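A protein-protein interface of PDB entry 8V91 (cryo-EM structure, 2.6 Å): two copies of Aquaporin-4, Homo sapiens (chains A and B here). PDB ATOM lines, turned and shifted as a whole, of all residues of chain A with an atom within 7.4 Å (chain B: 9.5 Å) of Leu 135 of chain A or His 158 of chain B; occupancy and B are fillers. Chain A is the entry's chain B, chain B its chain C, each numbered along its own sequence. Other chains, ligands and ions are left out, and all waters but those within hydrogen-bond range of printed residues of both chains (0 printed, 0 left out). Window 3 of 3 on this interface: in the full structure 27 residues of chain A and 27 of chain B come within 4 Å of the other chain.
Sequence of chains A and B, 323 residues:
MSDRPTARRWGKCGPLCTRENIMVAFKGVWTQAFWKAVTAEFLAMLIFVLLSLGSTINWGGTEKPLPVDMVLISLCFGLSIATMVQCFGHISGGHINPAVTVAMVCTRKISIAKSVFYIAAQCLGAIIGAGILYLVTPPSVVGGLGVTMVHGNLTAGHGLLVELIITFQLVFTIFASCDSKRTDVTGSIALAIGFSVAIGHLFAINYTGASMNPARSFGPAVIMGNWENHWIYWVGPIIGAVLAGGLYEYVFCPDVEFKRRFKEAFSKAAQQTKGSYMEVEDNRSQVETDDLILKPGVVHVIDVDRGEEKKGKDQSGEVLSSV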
ATOM      1  N   GLY A 129      17.310  39.087   7.930  1.00  0.00           N
ATOM      2  CA  GLY A 129      16.310  38.034   7.834  1.00  0.00           C
ATOM      3  C   GLY A 129      16.450  37.199   6.576  1.00  0.00           C
ATOM      4  O   GLY A 129      16.334  35.973   6.619  1.00  0.00           O
ATOM      5  N   ALA A 130      16.694  37.851   5.438  1.00  0.00           N
ATOM      6  CA  ALA A 130      16.927  37.111   4.202  1.00  0.00           C
ATOM      7  C   ALA A 130      18.274  36.403   4.220  1.00  0.00           C
ATOM      8  O   ALA A 130      18.414  35.326   3.632  1.00  0.00           O
ATOM      9  CB  ALA A 130      16.834  38.048   2.999  1.00  0.00           C
ATOM     10  N   GLY A 131      19.274  36.994   4.879  1.00  0.00           N
ATOM     11  CA  GLY A 131      20.568  36.340   4.980  1.00  0.00           C
ATOM     12  C   GLY A 131      20.504  35.035   5.750  1.00  0.00           C
ATOM     13  O   GLY A 131      21.155  34.055   5.380  1.00  0.00           O
ATOM     14  N   ILE A 132      19.726  35.006   6.834  1.00  0.00           N
ATOM     15  CA  ILE A 132      19.557  33.771   7.596  1.00  0.00           C
ATOM     16  C   ILE A 132      18.892  32.706   6.735  1.00  0.00           C
ATOM     17  O   ILE A 132      19.302  31.539   6.738  1.00  0.00           O
ATOM     18  CB  ILE A 132      18.757  34.038   8.884  1.00  0.00           C
ATOM     19  CG1 ILE A 132      19.544  34.942   9.830  1.00  0.00           C
ATOM     20  CG2 ILE A 132      18.420  32.733   9.581  1.00  0.00           C
ATOM     21  CD1 ILE A 132      18.705  35.529  10.939  1.00  0.00           C
ATOM     22  N   LEU A 133      17.857  33.090   5.983  1.00  0.00           N
ATOM     23  CA  LEU A 133      17.178  32.136   5.113  1.00  0.00           C
ATOM     24  C   LEU A 133      18.127  31.572   4.067  1.00  0.00           C
ATOM     25  O   LEU A 133      18.085  30.374   3.760  1.00  0.00           O
ATOM     26  CB  LEU A 133      15.975  32.798   4.441  1.00  0.00           C
ATOM     27  CG  LEU A 133      15.141  31.896   3.529  1.00  0.00           C
ATOM     28  CD1 LEU A 133      14.441  30.817   4.335  1.00  0.00           C
ATOM     29  CD2 LEU A 133      14.139  32.715   2.741  1.00  0.00           C
ATOM     30  N   TYR A 134      18.988  32.420   3.503  1.00  0.00           N
ATOM     31  CA  TYR A 134      19.978  31.939   2.548  1.00  0.00           C
ATOM     32  C   TYR A 134      20.948  30.962   3.196  1.00  0.00           C
ATOM     33  O   TYR A 134      21.501  30.090   2.516  1.00  0.00           O
ATOM     34  CB  TYR A 134      20.735  33.121   1.941  1.00  0.00           C
ATOM     35  CG  TYR A 134      21.774  32.726   0.922  1.00  0.00           C
ATOM     36  CD1 TYR A 134      21.402  32.282  -0.340  1.00  0.00           C
ATOM     37  CD2 TYR A 134      23.127  32.796   1.219  1.00  0.00           C
ATOM     38  CE1 TYR A 134      22.349  31.919  -1.276  1.00  0.00           C
ATOM     39  CE2 TYR A 134      24.081  32.434   0.289  1.00  0.00           C
ATOM     40  CZ  TYR A 134      23.686  31.997  -0.957  1.00  0.00           C
ATOM     41  OH  TYR A 134      24.632  31.636  -1.888  1.00  0.00           O
ATOM     42  N   LEU A 135      21.164  31.086   4.506  1.00  0.00           N
ATOM     43  CA  LEU A 135      22.080  30.194   5.205  1.00  0.00           C
ATOM     44  C   LEU A 135      21.461  28.824   5.456  1.00  0.00           C
ATOM     45  O   LEU A 135      22.158  27.806   5.392  1.00  0.00           O
ATOM     46  CB  LEU A 135      22.516  30.827   6.526  1.00  0.00           C
ATOM     47  CG  LEU A 135      23.976  30.631   6.928  1.00  0.00           C
ATOM     48  CD1 LEU A 135      24.877  31.546   6.113  1.00  0.00           C
ATOM     49  CD2 LEU A 135      24.155  30.881   8.415  1.00  0.00           C
ATOM     50  N   VAL A 136      20.157  28.776   5.741  1.00  0.00           N
ATOM     51  CA  VAL A 136      19.494  27.539   6.134  1.00  0.00           C
ATOM     52  C   VAL A 136      18.783  26.857   4.975  1.00  0.00           C
ATOM     53  O   VAL A 136      18.120  25.833   5.184  1.00  0.00           O
ATOM     54  CB  VAL A 136      18.502  27.788   7.287  1.00  0.00           C
ATOM     55  CG1 VAL A 136      19.223  28.378   8.486  1.00  0.00           C
ATOM     56  CG2 VAL A 136      17.383  28.706   6.834  1.00  0.00           C
ATOM     57  N   THR A 137      18.894  27.389   3.763  1.00  0.00           N
ATOM     58  CA  THR A 137      18.223  26.781   2.620  1.00  0.00           C
ATOM     59  C   THR A 137      19.218  25.986   1.793  1.00  0.00           C
ATOM     60  O   THR A 137      20.312  26.492   1.504  1.00  0.00           O
ATOM     61  CB  THR A 137      17.567  27.852   1.752  1.00  0.00           C
ATOM     62  OG1 THR A 137      16.628  28.596   2.540  1.00  0.00           O
ATOM     63  CG2 THR A 137      16.834  27.222   0.580  1.00  0.00           C
ATOM     64  N   PRO A 138      18.895  24.751   1.413  1.00  0.00           N
ATOM     65  CA  PRO A 138      19.798  23.968   0.559  1.00  0.00           C
ATOM     66  C   PRO A 138      20.049  24.673  -0.761  1.00  0.00           C
ATOM     67  O   PRO A 138      19.137  25.295  -1.326  1.00  0.00           O
ATOM     68  CB  PRO A 138      19.037  22.651   0.354  1.00  0.00           C
ATOM     69  CG  PRO A 138      18.123  22.560   1.526  1.00  0.00           C
ATOM     70  CD  PRO A 138      17.727  23.967   1.847  1.00  0.00           C
ATOM     71  N   PRO A 139      21.275  24.598  -1.284  1.00  0.00           N
ATOM     72  CA  PRO A 139      21.618  25.385  -2.480  1.00  0.00           C
ATOM     73  C   PRO A 139      20.772  25.069  -3.701  1.00  0.00           C
ATOM     74  O   PRO A 139      20.539  25.961  -4.526  1.00  0.00           O
ATOM     75  CB  PRO A 139      23.091  25.021  -2.706  1.00  0.00           C
ATOM     76  CG  PRO A 139      23.585  24.719  -1.328  1.00  0.00           C
ATOM     77  CD  PRO A 139      22.459  23.909  -0.747  1.00  0.00           C
ATOM     78  N   VAL A 142      17.335  27.121  -3.455  1.00  0.00           N
ATOM     79  CA  VAL A 142      17.336  28.535  -3.091  1.00  0.00           C
ATOM     80  C   VAL A 142      16.559  29.348  -4.118  1.00  0.00           C
ATOM     81  O   VAL A 142      15.706  30.171  -3.770  1.00  0.00           O
ATOM     82  CB  VAL A 142      18.779  29.049  -2.940  1.00  0.00           C
ATOM     83  CG1 VAL A 142      18.798  30.563  -2.913  1.00  0.00           C
ATOM     84  CG2 VAL A 142      19.418  28.489  -1.684  1.00  0.00           C
ATOM     85  N   LEU A 145      15.202  33.331  -3.984  1.00  0.00           N
ATOM     86  CA  LEU A 145      15.135  33.789  -2.595  1.00  0.00           C
ATOM     87  C   LEU A 145      13.996  34.783  -2.379  1.00  0.00           C
ATOM     88  O   LEU A 145      14.115  35.721  -1.587  1.00  0.00           O
ATOM     89  CB  LEU A 145      16.470  34.392  -2.145  1.00  0.00           C
ATOM     90  CG  LEU A 145      16.792  34.396  -0.649  1.00  0.00           C
ATOM     91  CD1 LEU A 145      17.241  33.018  -0.191  1.00  0.00           C
ATOM     92  CD2 LEU A 145      17.847  35.442  -0.333  1.00  0.00           C
ATOM     93  N   ILE A 223      20.907  40.632  -0.709  1.00  0.00           N
ATOM     94  CA  ILE A 223      21.592  39.354  -0.540  1.00  0.00           C
ATOM     95  C   ILE A 223      21.882  38.716  -1.893  1.00  0.00           C
ATOM     96  O   ILE A 223      22.989  38.229  -2.145  1.00  0.00           O
ATOM     97  CB  ILE A 223      20.762  38.420   0.358  1.00  0.00           C
ATOM     98  CG1 ILE A 223      20.584  39.037   1.747  1.00  0.00           C
ATOM     99  CG2 ILE A 223      21.413  37.049   0.452  1.00  0.00           C
ATOM    100  CD1 ILE A 223      21.883  39.342   2.449  1.00  0.00           C
ATOM    101  N   VAL B 150      14.447  15.866   9.456  1.00  0.00           N
ATOM    102  CA  VAL B 150      15.190  16.933   8.804  1.00  0.00           C
ATOM    103  C   VAL B 150      15.360  16.586   7.328  1.00  0.00           C
ATOM    104  O   VAL B 150      15.419  15.411   6.944  1.00  0.00           O
ATOM    105  CB  VAL B 150      16.551  17.140   9.496  1.00  0.00           C
ATOM    106  CG1 VAL B 150      17.340  18.268   8.844  1.00  0.00           C
ATOM    107  CG2 VAL B 150      16.359  17.413  10.975  1.00  0.00           C
ATOM    108  N   HIS B 151      15.424  17.617   6.488  1.00  0.00           N
ATOM    109  CA  HIS B 151      15.612  17.408   5.060  1.00  0.00           C
ATOM    110  C   HIS B 151      16.932  16.693   4.794  1.00  0.00           C
ATOM    111  O   HIS B 151      17.914  16.860   5.521  1.00  0.00           O
ATOM    112  CB  HIS B 151      15.577  18.744   4.318  1.00  0.00           C
ATOM    113  CG  HIS B 151      15.287  18.614   2.855  1.00  0.00           C
ATOM    114  ND1 HIS B 151      16.267  18.348   1.924  1.00  0.00           N
ATOM    115  CD2 HIS B 151      14.127  18.710   2.165  1.00  0.00           C
ATOM    116  CE1 HIS B 151      15.723  18.288   0.722  1.00  0.00           C
ATOM    117  NE2 HIS B 151      14.426  18.505   0.840  1.00  0.00           N
ATOM    118  N   ASN B 153      19.127  17.061   2.426  1.00  0.00           N
ATOM    119  CA  ASN B 153      20.206  17.970   2.065  1.00  0.00           C
ATOM    120  C   ASN B 153      20.445  19.053   3.107  1.00  0.00           C
ATOM    121  O   ASN B 153      21.286  19.929   2.883  1.00  0.00           O
ATOM    122  CB  ASN B 153      19.921  18.630   0.713  1.00  0.00           C
ATOM    123  CG  ASN B 153      19.531  17.630  -0.354  1.00  0.00           C
ATOM    124  OD1 ASN B 153      19.859  16.448  -0.266  1.00  0.00           O
ATOM    125  ND2 ASN B 153      18.825  18.102  -1.375  1.00  0.00           N
ATOM    126  N   LEU B 154      19.734  19.020   4.228  1.00  0.00           N
ATOM    127  CA  LEU B 154      19.841  20.049   5.253  1.00  0.00           C
ATOM    128  C   LEU B 154      20.650  19.516   6.429  1.00  0.00           C
ATOM    129  O   LEU B 154      20.386  18.416   6.923  1.00  0.00           O
ATOM    130  CB  LEU B 154      18.457  20.496   5.720  1.00  0.00           C
ATOM    131  CG  LEU B 154      18.428  21.551   6.825  1.00  0.00           C
ATOM    132  CD1 LEU B 154      19.052  22.837   6.324  1.00  0.00           C
ATOM    133  CD2 LEU B 154      17.011  21.796   7.300  1.00  0.00           C
ATOM    134  N   THR B 155      21.633  20.296   6.865  1.00  0.00           N
ATOM    135  CA  THR B 155      22.454  19.910   8.004  1.00  0.00           C
ATOM    136  C   THR B 155      21.653  20.035   9.295  1.00  0.00           C
ATOM    137  O   THR B 155      20.862  20.967   9.464  1.00  0.00           O
ATOM    138  CB  THR B 155      23.711  20.781   8.064  1.00  0.00           C
ATOM    139  OG1 THR B 155      24.537  20.504   6.928  1.00  0.00           O
ATOM    140  CG2 THR B 155      24.510  20.504   9.327  1.00  0.00           C
ATOM    141  N   ALA B 156      21.854  19.078  10.208  1.00  0.00           N
ATOM    142  CA  ALA B 156      21.149  19.112  11.485  1.00  0.00           C
ATOM    143  C   ALA B 156      21.477  20.369  12.279  1.00  0.00           C
ATOM    144  O   ALA B 156      20.665  20.814  13.097  1.00  0.00           O
ATOM    145  CB  ALA B 156      21.483  17.866  12.303  1.00  0.00           C
ATOM    146  N   GLY B 157      22.660  20.947  12.062  1.00  0.00           N
ATOM    147  CA  GLY B 157      22.982  22.209  12.709  1.00  0.00           C
ATOM    148  C   GLY B 157      22.059  23.332  12.280  1.00  0.00           C
ATOM    149  O   GLY B 157      21.612  24.131  13.106  1.00  0.00           O
ATOM    150  N   HIS B 158      21.765  23.413  10.981  1.00  0.00           N
ATOM    151  CA  HIS B 158      20.774  24.374  10.509  1.00  0.00           C
ATOM    152  C   HIS B 158      19.369  23.983  10.944  1.00  0.00           C
ATOM    153  O   HIS B 158      18.499  24.850  11.080  1.00  0.00           O
ATOM    154  CB  HIS B 158      20.839  24.500   8.989  1.00  0.00           C
ATOM    155  CG  HIS B 158      22.142  25.031   8.481  1.00  0.00           C
ATOM    156  ND1 HIS B 158      22.800  24.479   7.402  1.00  0.00           N
ATOM    157  CD2 HIS B 158      22.908  26.065   8.901  1.00  0.00           C
ATOM    158  CE1 HIS B 158      23.917  25.149   7.181  1.00  0.00           C
ATOM    159  NE2 HIS B 158      24.005  26.116   8.077  1.00  0.00           N
ATOM    160  N   GLY B 159      19.126  22.688  11.154  1.00  0.00           N
ATOM    161  CA  GLY B 159      17.825  22.261  11.637  1.00  0.00           C
ATOM    162  C   GLY B 159      17.537  22.752  13.041  1.00  0.00           C
ATOM    163  O   GLY B 159      16.398  23.092  13.369  1.00  0.00           O
ATOM    164  N   LEU B 160      18.563  22.786  13.893  1.00  0.00           N
ATOM    165  CA  LEU B 160      18.394  23.320  15.240  1.00  0.00           C
ATOM    166  C   LEU B 160      18.065  24.806  15.205  1.00  0.00           C
ATOM    167  O   LEU B 160      17.243  25.288  15.992  1.00  0.00           O
ATOM    168  CB  LEU B 160      19.660  23.072  16.059  1.00  0.00           C
ATOM    169  CG  LEU B 160      19.593  23.417  17.544  1.00  0.00           C
ATOM    170  CD1 LEU B 160      18.799  22.364  18.285  1.00  0.00           C
ATOM    171  CD2 LEU B 160      20.989  23.544  18.123  1.00  0.00           C
ATOM    172  N   LEU B 161      18.703  25.548  14.297  1.00  0.00           N
ATOM    173  CA  LEU B 161      18.460  26.984  14.202  1.00  0.00           C
ATOM    174  C   LEU B 161      17.025  27.278  13.783  1.00  0.00           C
ATOM    175  O   LEU B 161      16.409  28.229  14.278  1.00  0.00           O
ATOM    176  CB  LEU B 161      19.445  27.613  13.219  1.00  0.00           C
ATOM    177  CG  LEU B 161      19.311  29.117  12.982  1.00  0.00           C
ATOM    178  CD1 LEU B 161      19.486  29.881  14.282  1.00  0.00           C
ATOM    179  CD2 LEU B 161      20.317  29.581  11.946  1.00  0.00           C
ATOM    180  N   VAL B 162      16.479  26.478  12.865  1.00  0.00           N
ATOM    181  CA  VAL B 162      15.112  26.702  12.404  1.00  0.00           C
ATOM    182  C   VAL B 162      14.123  26.508  13.547  1.00  0.00           C
ATOM    183  O   VAL B 162      13.203  27.313  13.735  1.00  0.00           O
ATOM    184  CB  VAL B 162      14.795  25.781  11.212  1.00  0.00           C
ATOM    185  CG1 VAL B 162      13.309  25.795  10.911  1.00  0.00           C
ATOM    186  CG2 VAL B 162      15.595  26.197   9.991  1.00  0.00           C
ATOM    187  N   GLU B 163      14.299  25.440  14.332  1.00  0.00           N
ATOM    188  CA  GLU B 163      13.447  25.222  15.498  1.00  0.00           C
ATOM    189  C   GLU B 163      13.615  26.323  16.534  1.00  0.00           C
ATOM    190  O   GLU B 163      12.649  26.693  17.209  1.00  0.00           O
ATOM    191  CB  GLU B 163      13.750  23.863  16.131  1.00  0.00           C
ATOM    192  CG  GLU B 163      12.706  22.805  15.859  1.00  0.00           C
ATOM    193  CD  GLU B 163      12.515  22.559  14.385  1.00  0.00           C
ATOM    194  OE1 GLU B 163      13.530  22.412  13.675  1.00  0.00           O
ATOM    195  OE2 GLU B 163      11.353  22.506  13.933  1.00  0.00           O
ATOM    196  N   LEU B 164      14.834  26.845  16.682  1.00  0.00           N
ATOM    197  CA  LEU B 164      15.077  27.914  17.642  1.00  0.00           C
ATOM    198  C   LEU B 164      14.249  29.151  17.324  1.00  0.00           C
ATOM    199  O   LEU B 164      13.880  29.901  18.234  1.00  0.00           O
ATOM    200  CB  LEU B 164      16.571  28.248  17.666  1.00  0.00           C
ATOM    201  CG  LEU B 164      17.157  29.260  18.653  1.00  0.00           C
ATOM    202  CD1 LEU B 164      18.615  28.928  18.897  1.00  0.00           C
ATOM    203  CD2 LEU B 164      17.039  30.686  18.139  1.00  0.00           C
ATOM    204  N   ILE B 165      13.939  29.378  16.050  1.00  0.00           N
ATOM    205  CA  ILE B 165      13.275  30.611  15.642  1.00  0.00           C
ATOM    206  C   ILE B 165      11.762  30.440  15.558  1.00  0.00           C
ATOM    207  O   ILE B 165      11.012  31.310  16.007  1.00  0.00           O
ATOM    208  CB  ILE B 165      13.870  31.102  14.308  1.00  0.00           C
ATOM    209  CG1 ILE B 165      15.328  31.519  14.510  1.00  0.00           C
ATOM    210  CG2 ILE B 165      13.062  32.258  13.751  1.00  0.00           C
ATOM    211  CD1 ILE B 165      16.043  31.899  13.239  1.00  0.00           C
ATOM    212  N   ILE B 166      11.281  29.329  14.992  1.00  0.00           N
ATOM    213  CA  ILE B 166       9.836  29.147  14.869  1.00  0.00           C
ATOM    214  C   ILE B 166       9.189  28.998  16.240  1.00  0.00           C
ATOM    215  O   ILE B 166       8.024  29.368  16.426  1.00  0.00           O
ATOM    216  CB  ILE B 166       9.505  27.951  13.956  1.00  0.00           C
ATOM    217  CG1 ILE B 166      10.099  26.657  14.514  1.00  0.00           C
ATOM    218  CG2 ILE B 166      10.002  28.208  12.543  1.00  0.00           C
ATOM    219  CD1 ILE B 166       9.824  25.450  13.654  1.00  0.00           C
ATOM    220  N   PHE B 203       6.241  27.547   6.948  1.00  0.00           N
ATOM    221  CA  PHE B 203       7.647  27.776   6.646  1.00  0.00           C
ATOM    222  C   PHE B 203       8.491  26.511   6.710  1.00  0.00           C
ATOM    223  O   PHE B 203       9.187  26.185   5.745  1.00  0.00           O
ATOM    224  CB  PHE B 203       8.212  28.821   7.619  1.00  0.00           C
ATOM    225  CG  PHE B 203       9.709  28.955   7.576  1.00  0.00           C
ATOM    226  CD1 PHE B 203      10.387  29.035   6.372  1.00  0.00           C
ATOM    227  CD2 PHE B 203      10.440  28.992   8.750  1.00  0.00           C
ATOM    228  CE1 PHE B 203      11.762  29.153   6.345  1.00  0.00           C
ATOM    229  CE2 PHE B 203      11.812  29.110   8.728  1.00  0.00           C
ATOM    230  CZ  PHE B 203      12.474  29.191   7.525  1.00  0.00           C
ATOM    231  N   ALA B 204       8.444  25.780   7.824  1.00  0.00           N
ATOM    232  CA  ALA B 204       9.477  24.809   8.162  1.00  0.00           C
ATOM    233  C   ALA B 204       8.989  23.363   8.145  1.00  0.00           C
ATOM    234  O   ALA B 204       9.458  22.543   8.936  1.00  0.00           O
ATOM    235  CB  ALA B 204      10.075  25.140   9.527  1.00  0.00           C
ATOM    236  N   TYR B 207      11.926  21.799   6.106  1.00  0.00           N
ATOM    237  CA  TYR B 207      13.223  21.931   6.756  1.00  0.00           C
ATOM    238  C   TYR B 207      13.403  20.857   7.821  1.00  0.00           C
ATOM    239  O   TYR B 207      14.312  20.026   7.738  1.00  0.00           O
ATOM    240  CB  TYR B 207      13.369  23.327   7.368  1.00  0.00           C
ATOM    241  CG  TYR B 207      13.519  24.439   6.356  1.00  0.00           C
ATOM    242  CD1 TYR B 207      12.414  24.958   5.697  1.00  0.00           C
ATOM    243  CD2 TYR B 207      14.765  24.969   6.059  1.00  0.00           C
ATOM    244  CE1 TYR B 207      12.546  25.977   4.778  1.00  0.00           C
ATOM    245  CE2 TYR B 207      14.907  25.985   5.137  1.00  0.00           C
ATOM    246  CZ  TYR B 207      13.794  26.484   4.500  1.00  0.00           C
ATOM    247  OH  TYR B 207      13.932  27.497   3.580  1.00  0.00           O
ATOM    248  N   THR B 208      12.532  20.858   8.834  1.00  0.00           N
ATOM    249  CA  THR B 208      12.612  19.879   9.910  1.00  0.00           C
ATOM    250  C   THR B 208      11.256  19.290  10.277  1.00  0.00           C
ATOM    251  O   THR B 208      11.169  18.552  11.265  1.00  0.00           O
ATOM    252  CB  THR B 208      13.238  20.498  11.163  1.00  0.00           C
ATOM    253  OG1 THR B 208      12.405  21.565  11.630  1.00  0.00           O
ATOM    254  CG2 THR B 208      14.624  21.035  10.874  1.00  0.00           C
ATOM    255  N   TRP B 231      17.300  15.007  19.247  1.00  0.00           N
ATOM    256  CA  TRP B 231      17.761  15.975  20.236  1.00  0.00           C
ATOM    257  C   TRP B 231      17.507  17.408  19.786  1.00  0.00           C
ATOM    258  O   TRP B 231      17.319  18.294  20.627  1.00  0.00           O
ATOM    259  CB  TRP B 231      19.247  15.757  20.529  1.00  0.00           C
ATOM    260  CG  TRP B 231      20.142  16.010  19.357  1.00  0.00           C
ATOM    261  CD1 TRP B 231      20.534  15.106  18.416  1.00  0.00           C
ATOM    262  CD2 TRP B 231      20.764  17.251  19.007  1.00  0.00           C
ATOM    263  NE1 TRP B 231      21.358  15.707  17.497  1.00  0.00           N
ATOM    264  CE2 TRP B 231      21.517  17.024  17.838  1.00  0.00           C
ATOM    265  CE3 TRP B 231      20.756  18.532  19.566  1.00  0.00           C
ATOM    266  CZ2 TRP B 231      22.252  18.031  17.218  1.00  0.00           C
ATOM    267  CZ3 TRP B 231      21.487  19.529  18.950  1.00  0.00           C
ATOM    268  CH2 TRP B 231      22.225  19.273  17.789  1.00  0.00           C
ATOM    269  N   ILE B 232      17.496  17.660  18.474  1.00  0.00           N
ATOM    270  CA  ILE B 232      17.228  19.007  17.989  1.00  0.00           C
ATOM    271  C   ILE B 232      15.782  19.412  18.232  1.00  0.00           C
ATOM    272  O   ILE B 232      15.457  20.603  18.171  1.00  0.00           O
ATOM    273  CB  ILE B 232      17.576  19.135  16.494  1.00  0.00           C
ATOM    274  CG1 ILE B 232      16.452  18.570  15.627  1.00  0.00           C
ATOM    275  CG2 ILE B 232      18.876  18.428  16.185  1.00  0.00           C
ATOM    276  CD1 ILE B 232      16.414  19.150  14.238  1.00  0.00           C
ATOM    277  N   TYR B 233      14.900  18.450  18.502  1.00  0.00           N
ATOM    278  CA  TYR B 233      13.494  18.734  18.742  1.00  0.00           C
ATOM    279  C   TYR B 233      13.187  18.982  20.211  1.00  0.00           C
ATOM    280  O   TYR B 233      12.061  19.370  20.537  1.00  0.00           O
ATOM    281  CB  TYR B 233      12.639  17.583  18.212  1.00  0.00           C
ATOM    282  CG  TYR B 233      12.679  17.485  16.707  1.00  0.00           C
ATOM    283  CD1 TYR B 233      12.351  18.578  15.916  1.00  0.00           C
ATOM    284  CD2 TYR B 233      13.071  16.313  16.076  1.00  0.00           C
ATOM    285  CE1 TYR B 233      12.395  18.500  14.541  1.00  0.00           C
ATOM    286  CE2 TYR B 233      13.119  16.228  14.700  1.00  0.00           C
ATOM    287  CZ  TYR B 233      12.779  17.325  13.938  1.00  0.00           C
ATOM    288  OH  TYR B 233      12.822  17.250  12.566  1.00  0.00           O
ATOM    289  N   GLY B 236      16.132  22.465  20.607  1.00  0.00           N
ATOM    290  CA  GLY B 236      15.729  23.554  19.751  1.00  0.00           C
ATOM    291  C   GLY B 236      14.618  24.406  20.328  1.00  0.00           C
ATOM    292  O   GLY B 236      14.816  25.583  20.649  1.00  0.00           O
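The side-chain hydroxyl (OG1) of Thr 137 of chain A is in hydrogen-bond range of the side-chain hydroxyl (OH) of Tyr 207 of chain B (3.1 Å).
O of Leu 133 of chain A is in hydrogen-bond range of OG1 of Thr 137 of chain A (2.6 Å).
O of Tyr 207 of chain B is in hydrogen-bond range of N of His 151 of chain B.
Among the printed residues, pairs that only touch across the chains: Val 136 of chain A with Tyr 207 of chain B, Val 136 of chain A with Leu 154 of chain B, Leu 133 of chain A with Tyr 207 of chain B, Leu 135 of chain A with His 158 of chain B, Leu 133 of chain A with Phe 203 of chain B and Val 136 of chain A with Leu 161 of chain B.
Printed residues of chain B within 4 Å of Leu 133 of chain A: Phe 203 and Tyr 207.
Of chain B, only His 158 comes within 4 Å of Leu 135 of chain A.
Val 136 of chain A touches three residues of chain B.
Val 142 of chain A touches none of the printed residues of chain B.
Of the printed residues of chain A, Leu 154 of chain B touches Val 136 (3.3 Å).
No residue of chain A comes within 4 Å of Gly 157 of chain B.
His 158 of chain B touches one residue of chain A.
Glu 163 of chain B touches none of the printed residues of chain A.
The nearest residue of chain B that does not touch Leu 135 of chain A is Leu 161 of chain B (5.4 Å).
The nearest printed residue of chain A that does not touch Leu 161 of chain B is Ile 132 of chain A (4.4 Å).
Of the 24 printed residues of chain B, 5 touch a printed residue of chain A.
Of the 14 printed residues of chain A, 4 touch a printed residue of chain B.
Along chain A the printed residues that touch a printed residue of chain B span positions 133 to 137.
Among the printed residues, no Asp or Glu carboxylate lies within 4 Å of a Lys or Arg side-chain nitrogen of the other chain.
No position is printed for both chains.
Of the 7 pairs that touch across the chains among the printed residues, none has its exchanged pair printed and touching as well.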
